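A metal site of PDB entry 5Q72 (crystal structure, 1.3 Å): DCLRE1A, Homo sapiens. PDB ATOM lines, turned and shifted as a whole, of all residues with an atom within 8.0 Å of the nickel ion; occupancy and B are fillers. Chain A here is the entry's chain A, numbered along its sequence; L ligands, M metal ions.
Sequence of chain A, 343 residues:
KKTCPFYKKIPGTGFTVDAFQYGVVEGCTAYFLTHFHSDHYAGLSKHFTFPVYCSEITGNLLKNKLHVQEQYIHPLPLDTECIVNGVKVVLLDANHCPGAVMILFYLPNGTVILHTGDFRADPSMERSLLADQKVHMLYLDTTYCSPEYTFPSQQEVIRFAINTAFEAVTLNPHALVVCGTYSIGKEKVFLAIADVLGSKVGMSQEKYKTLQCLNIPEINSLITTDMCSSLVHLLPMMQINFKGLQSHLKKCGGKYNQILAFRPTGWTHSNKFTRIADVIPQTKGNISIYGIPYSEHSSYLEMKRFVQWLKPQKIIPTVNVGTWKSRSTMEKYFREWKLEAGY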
ATOM      1  N   ASP A  18      21.445  -8.404   4.144  1.00  0.00           N
ATOM      2  CA  ASP A  18      22.049  -9.646   4.701  1.00  0.00           C
ATOM      3  C   ASP A  18      23.494  -9.389   5.314  1.00  0.00           C
ATOM      4  O   ASP A  18      24.452 -10.200   5.124  1.00  0.00           O
ATOM      5  CB  ASP A  18      21.969 -10.791   3.754  1.00  0.00           C
ATOM      6  CG  ASP A  18      20.520 -11.145   3.282  1.00  0.00           C
ATOM      7  OD1 ASP A  18      19.569 -10.728   3.954  1.00  0.00           O
ATOM      8  OD2 ASP A  18      20.510 -11.955   2.324  1.00  0.00           O
ATOM      9  N   THR A  34      16.770 -10.910   3.739  1.00  0.00           N
ATOM     10  CA  THR A  34      16.012 -11.607   2.689  1.00  0.00           C
ATOM     11  C   THR A  34      15.281 -12.880   3.216  1.00  0.00           C
ATOM     12  O   THR A  34      14.201 -13.169   2.717  1.00  0.00           O
ATOM     13  CB  THR A  34      16.867 -11.939   1.459  1.00  0.00           C
ATOM     14  OG1 THR A  34      17.937 -12.867   1.831  1.00  0.00           O
ATOM     15  CG2 THR A  34      17.472 -10.672   0.822  1.00  0.00           C
ATOM     16  N   HIS A  35      15.932 -13.647   4.115  1.00  0.00           N
ATOM     17  CA  HIS A  35      15.364 -14.895   4.593  1.00  0.00           C
ATOM     18  C   HIS A  35      16.031 -15.324   5.863  1.00  0.00           C
ATOM     19  O   HIS A  35      17.225 -14.947   6.083  1.00  0.00           O
ATOM     20  CB  HIS A  35      15.327 -15.964   3.441  1.00  0.00           C
ATOM     21  CG  HIS A  35      16.656 -16.484   2.980  1.00  0.00           C
ATOM     22  ND1 HIS A  35      17.614 -15.742   2.311  1.00  0.00           N
ATOM     23  CD2 HIS A  35      17.201 -17.726   3.109  1.00  0.00           C
ATOM     24  CE1 HIS A  35      18.639 -16.541   1.987  1.00  0.00           C
ATOM     25  NE2 HIS A  35      18.385 -17.742   2.429  1.00  0.00           N
ATOM     26  N   PHE A  36      15.388 -16.258   6.525  1.00  0.00           N
ATOM     27  CA  PHE A  36      15.952 -16.848   7.806  1.00  0.00           C
ATOM     28  C   PHE A  36      16.833 -18.074   7.622  1.00  0.00           C
ATOM     29  O   PHE A  36      16.379 -19.218   8.006  1.00  0.00           O
ATOM     30  CB  PHE A  36      14.776 -17.138   8.825  1.00  0.00           C
ATOM     31  CG  PHE A  36      15.188 -17.325  10.266  1.00  0.00           C
ATOM     32  CD1 PHE A  36      15.574 -16.232  11.055  1.00  0.00           C
ATOM     33  CD2 PHE A  36      15.173 -18.600  10.841  1.00  0.00           C
ATOM     34  CE1 PHE A  36      15.873 -16.462  12.419  1.00  0.00           C
ATOM     35  CE2 PHE A  36      15.507 -18.826  12.179  1.00  0.00           C
ATOM     36  CZ  PHE A  36      15.856 -17.778  12.942  1.00  0.00           C
ATOM     37  N   HIS A  37      17.986 -17.935   6.930  1.00  0.00           N
ATOM     38  CA  HIS A  37      19.068 -18.918   6.878  1.00  0.00           C
ATOM     39  C   HIS A  37      20.315 -18.324   7.570  1.00  0.00           C
ATOM     40  O   HIS A  37      20.671 -17.153   7.391  1.00  0.00           O
ATOM     41  CB  HIS A  37      19.380 -19.416   5.433  1.00  0.00           C
ATOM     42  CG  HIS A  37      18.402 -20.438   4.863  1.00  0.00           C
ATOM     43  ND1 HIS A  37      18.340 -20.759   3.517  1.00  0.00           N
ATOM     44  CD2 HIS A  37      17.543 -21.267   5.489  1.00  0.00           C
ATOM     45  CE1 HIS A  37      17.488 -21.755   3.335  1.00  0.00           C
ATOM     46  NE2 HIS A  37      16.956 -22.047   4.525  1.00  0.00           N
ATOM     47  N   SER A  38      21.020 -19.199   8.331  1.00  0.00           N
ATOM     48  CA  SER A  38      22.058 -18.719   9.238  1.00  0.00           C
ATOM     49  C   SER A  38      23.182 -17.989   8.550  1.00  0.00           C
ATOM     50  O   SER A  38      23.672 -17.006   9.146  1.00  0.00           O
ATOM     51  CB  SER A  38      22.469 -19.844  10.193  1.00  0.00           C
ATOM     52  OG  SER A  38      23.101 -20.872   9.471  1.00  0.00           O
ATOM     53  N   ASP A  39      23.571 -18.333   7.306  1.00  0.00           N
ATOM     54  CA  ASP A  39      24.678 -17.596   6.633  1.00  0.00           C
ATOM     55  C   ASP A  39      24.256 -16.150   6.373  1.00  0.00           C
ATOM     56  O   ASP A  39      25.135 -15.279   6.287  1.00  0.00           O
ATOM     57  CB  ASP A  39      25.152 -18.231   5.350  1.00  0.00           C
ATOM     58  CG  ASP A  39      26.126 -19.476   5.585  1.00  0.00           C
ATOM     59  OD1 ASP A  39      26.486 -19.733   6.750  1.00  0.00           O
ATOM     60  OD2 ASP A  39      26.407 -20.144   4.573  1.00  0.00           O
ATOM     61  N   HIS A  40      22.940 -15.873   6.268  1.00  0.00           N
ATOM     62  CA  HIS A  40      22.425 -14.541   5.919  1.00  0.00           C
ATOM     63  C   HIS A  40      22.049 -13.768   7.150  1.00  0.00           C
ATOM     64  O   HIS A  40      22.314 -12.520   7.176  1.00  0.00           O
ATOM     65  CB  HIS A  40      21.178 -14.711   4.968  1.00  0.00           C
ATOM     66  CG  HIS A  40      21.545 -15.331   3.678  1.00  0.00           C
ATOM     67  ND1 HIS A  40      21.706 -14.622   2.504  1.00  0.00           N
ATOM     68  CD2 HIS A  40      21.842 -16.626   3.365  1.00  0.00           C
ATOM     69  CE1 HIS A  40      22.148 -15.421   1.564  1.00  0.00           C
ATOM     70  NE2 HIS A  40      22.215 -16.652   2.052  1.00  0.00           N
ATOM     71  N   HIS A  96      12.147 -19.712  -2.549  1.00  0.00           N
ATOM     72  CA  HIS A  96      13.277 -20.343  -1.814  1.00  0.00           C
ATOM     73  C   HIS A  96      12.629 -21.042  -0.604  1.00  0.00           C
ATOM     74  O   HIS A  96      11.857 -22.027  -0.857  1.00  0.00           O
ATOM     75  CB  HIS A  96      14.364 -19.267  -1.498  1.00  0.00           C
ATOM     76  CG  HIS A  96      15.642 -19.759  -0.823  1.00  0.00           C
ATOM     77  ND1 HIS A  96      16.376 -20.828  -1.284  1.00  0.00           N
ATOM     78  CD2 HIS A  96      16.243 -19.371   0.334  1.00  0.00           C
ATOM     79  CE1 HIS A  96      17.460 -20.966  -0.513  1.00  0.00           C
ATOM     80  NE2 HIS A  96      17.377 -20.132   0.504  1.00  0.00           N
ATOM     81  N   CYS A  97      12.902 -20.685   0.618  1.00  0.00           N
ATOM     82  CA  CYS A  97      12.258 -21.252   1.829  1.00  0.00           C
ATOM     83  C   CYS A  97      11.090 -20.328   2.271  1.00  0.00           C
ATOM     84  O   CYS A  97      10.970 -19.205   1.771  1.00  0.00           O
ATOM     85  CB  CYS A  97      13.308 -21.341   2.955  1.00  0.00           C
ATOM     86  SG  CYS A  97      14.037 -19.765   3.488  1.00  0.00           S
ATOM     87  N   ALA A 100      11.121 -16.165   2.366  1.00  0.00           N
ATOM     88  CA  ALA A 100      12.225 -15.632   1.533  1.00  0.00           C
ATOM     89  C   ALA A 100      11.736 -14.697   0.461  1.00  0.00           C
ATOM     90  O   ALA A 100      10.714 -14.969  -0.199  1.00  0.00           O
ATOM     91  CB  ALA A 100      12.974 -16.764   0.910  1.00  0.00           C
ATOM     92  N   GLY A 117      18.199 -12.072  -3.265  1.00  0.00           N
ATOM     93  CA  GLY A 117      18.471 -12.946  -2.101  1.00  0.00           C
ATOM     94  C   GLY A 117      18.850 -14.298  -2.620  1.00  0.00           C
ATOM     95  O   GLY A 117      19.525 -14.409  -3.633  1.00  0.00           O
ATOM     96  N   ASP A 118      18.454 -15.353  -1.897  1.00  0.00           N
ATOM     97  CA  ASP A 118      18.497 -16.739  -2.446  1.00  0.00           C
ATOM     98  C   ASP A 118      17.149 -16.989  -3.167  1.00  0.00           C
ATOM     99  O   ASP A 118      16.070 -16.633  -2.639  1.00  0.00           O
ATOM    100  CB  ASP A 118      18.679 -17.771  -1.344  1.00  0.00           C
ATOM    101  CG  ASP A 118      20.134 -17.895  -0.823  1.00  0.00           C
ATOM    102  OD1 ASP A 118      21.069 -17.349  -1.423  1.00  0.00           O
ATOM    103  OD2 ASP A 118      20.339 -18.630   0.148  1.00  0.00           O
ATOM    104  N   PHE A 119      17.218 -17.575  -4.366  1.00  0.00           N
ATOM    105  CA  PHE A 119      15.964 -17.828  -5.141  1.00  0.00           C
ATOM    106  C   PHE A 119      16.052 -19.073  -6.019  1.00  0.00           C
ATOM    107  O   PHE A 119      17.147 -19.499  -6.392  1.00  0.00           O
ATOM    108  CB  PHE A 119      15.482 -16.572  -5.963  1.00  0.00           C
ATOM    109  CG  PHE A 119      16.107 -16.284  -7.367  1.00  0.00           C
ATOM    110  CD1 PHE A 119      15.315 -15.830  -8.424  1.00  0.00           C
ATOM    111  CD2 PHE A 119      17.500 -16.496  -7.631  1.00  0.00           C
ATOM    112  CE1 PHE A 119      15.838 -15.524  -9.684  1.00  0.00           C
ATOM    113  CE2 PHE A 119      17.991 -16.199  -8.897  1.00  0.00           C
ATOM    114  CZ  PHE A 119      17.177 -15.741  -9.908  1.00  0.00           C
ATOM    115  N   ASP A 141      21.747 -14.463  -7.069  1.00  0.00           N
ATOM    116  CA  ASP A 141      22.103 -15.767  -6.457  1.00  0.00           C
ATOM    117  C   ASP A 141      22.603 -16.692  -7.547  1.00  0.00           C
ATOM    118  O   ASP A 141      21.872 -17.273  -8.349  1.00  0.00           O
ATOM    119  CB  ASP A 141      20.893 -16.401  -5.774  1.00  0.00           C
ATOM    120  CG  ASP A 141      21.069 -17.837  -5.355  1.00  0.00           C
ATOM    121  OD1 ASP A 141      22.236 -18.295  -5.288  1.00  0.00           O
ATOM    122  OD2 ASP A 141      20.023 -18.488  -5.056  1.00  0.00           O
ATOM    123  N   THR A 143      24.477 -19.582  -7.000  1.00  0.00           N
ATOM    124  CA  THR A 143      24.897 -20.827  -6.390  1.00  0.00           C
ATOM    125  C   THR A 143      25.210 -21.888  -7.429  1.00  0.00           C
ATOM    126  O   THR A 143      26.313 -22.489  -7.293  1.00  0.00           O
ATOM    127  CB  THR A 143      23.755 -21.301  -5.373  1.00  0.00           C
ATOM    128  OG1 THR A 143      23.571 -20.428  -4.277  1.00  0.00           O
ATOM    129  CG2 THR A 143      24.185 -22.656  -4.833  1.00  0.00           C
ATOM    130  N   SER A 183      17.502 -26.675   8.907  1.00  0.00           N
ATOM    131  CA  SER A 183      17.127 -25.292   8.650  1.00  0.00           C
ATOM    132  C   SER A 183      15.672 -25.301   8.186  1.00  0.00           C
ATOM    133  O   SER A 183      15.099 -26.380   7.849  1.00  0.00           O
ATOM    134  CB  SER A 183      17.975 -24.632   7.502  1.00  0.00           C
ATOM    135  OG  SER A 183      17.909 -25.359   6.268  1.00  0.00           O
ATOM    136  N   ILE A 184      15.083 -24.158   8.052  1.00  0.00           N
ATOM    137  CA  ILE A 184      13.815 -24.048   7.353  1.00  0.00           C
ATOM    138  C   ILE A 184      14.016 -24.261   5.819  1.00  0.00           C
ATOM    139  O   ILE A 184      15.134 -24.140   5.287  1.00  0.00           O
ATOM    140  CB  ILE A 184      13.031 -22.741   7.634  1.00  0.00           C
ATOM    141  CG1 ILE A 184      13.715 -21.508   7.054  1.00  0.00           C
ATOM    142  CG2 ILE A 184      12.741 -22.637   9.116  1.00  0.00           C
ATOM    143  CD1 ILE A 184      12.898 -20.245   7.028  1.00  0.00           C
ATOM    144  N   GLU A 296      16.132 -25.775  -3.607  1.00  0.00           N
ATOM    145  CA  GLU A 296      15.488 -24.433  -3.486  1.00  0.00           C
ATOM    146  C   GLU A 296      16.349 -23.265  -4.077  1.00  0.00           C
ATOM    147  O   GLU A 296      16.197 -22.080  -3.742  1.00  0.00           O
ATOM    148  CB  GLU A 296      15.002 -24.159  -2.065  1.00  0.00           C
ATOM    149  CG  GLU A 296      13.804 -25.080  -1.594  1.00  0.00           C
ATOM    150  CD  GLU A 296      13.221 -24.784  -0.219  1.00  0.00           C
ATOM    151  OE1 GLU A 296      13.838 -24.173   0.664  1.00  0.00           O
ATOM    152  OE2 GLU A 296      12.029 -25.252  -0.056  1.00  0.00           O
ATOM    153  N   HIS A 297      17.319 -23.675  -4.898  1.00  0.00           N
ATOM    154  CA  HIS A 297      18.079 -22.711  -5.745  1.00  0.00           C
ATOM    155  C   HIS A 297      17.920 -22.984  -7.223  1.00  0.00           C
ATOM    156  O   HIS A 297      17.648 -24.172  -7.629  1.00  0.00           O
ATOM    157  CB  HIS A 297      19.612 -22.778  -5.436  1.00  0.00           C
ATOM    158  CG  HIS A 297      20.009 -22.319  -4.077  1.00  0.00           C
ATOM    159  ND1 HIS A 297      20.260 -20.994  -3.751  1.00  0.00           N
ATOM    160  CD2 HIS A 297      20.332 -23.025  -2.950  1.00  0.00           C
ATOM    161  CE1 HIS A 297      20.631 -20.904  -2.478  1.00  0.00           C
ATOM    162  NE2 HIS A 297      20.659 -22.117  -1.973  1.00  0.00           N
HETATM  163  C1  LIG L   1      21.629 -21.921   2.601  1.00  0.00           C
HETATM  164  C2  LIG L   1      21.017 -22.234   1.259  1.00  0.00           C
HETATM  165  C3  LIG L   1      21.911 -20.441   2.856  1.00  0.00           C
HETATM  166  O1  LIG L   1      21.415 -23.158   0.513  1.00  0.00           O
HETATM  167  O2  LIG L   1      20.028 -21.557   0.910  1.00  0.00           O
HETATM  168  O3  LIG L   1      21.032 -19.555   2.678  1.00  0.00           O
HETATM  169  O4  LIG L   1      23.044 -20.174   3.356  1.00  0.00           O
HETATM  170 NI    NI M   1      19.232 -19.700   1.742  1.00  0.00          NI
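A ring nitrogen (NE2) of His 37 is in hydrogen-bond range of the backbone carbonyl oxygen of Ile 184 (2.9 Å). ND1 of His 35 is in hydrogen-bond range of OG1 of Thr 34, at 2.9 Å. OD2 of Asp 118 lies close to NE2 of His 40 (3.3 Å). O of Glu 296 sits at hydrogen-bond distance from ND1 of His 96.
Within 4 Å of the nickel ion: His 35, His 37, His 96 and Asp 118.
The nickel ion is bound by an oxygen (O3) of the ligand. The nickel ion is bound by O2 of the ligand (2.2 Å). OD2 of Asp 118 is bound to the nickel ion, at 2.2 Å. NE2 of His 35 binds the nickel ion, at 2.2 Å. ND1 of His 37 binds the nickel ion (2.3 Å). The nickel ion is bound by a ring nitrogen (NE2) of His 96 (2.3 Å). The nickel ion has six donor atoms within binding distance.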
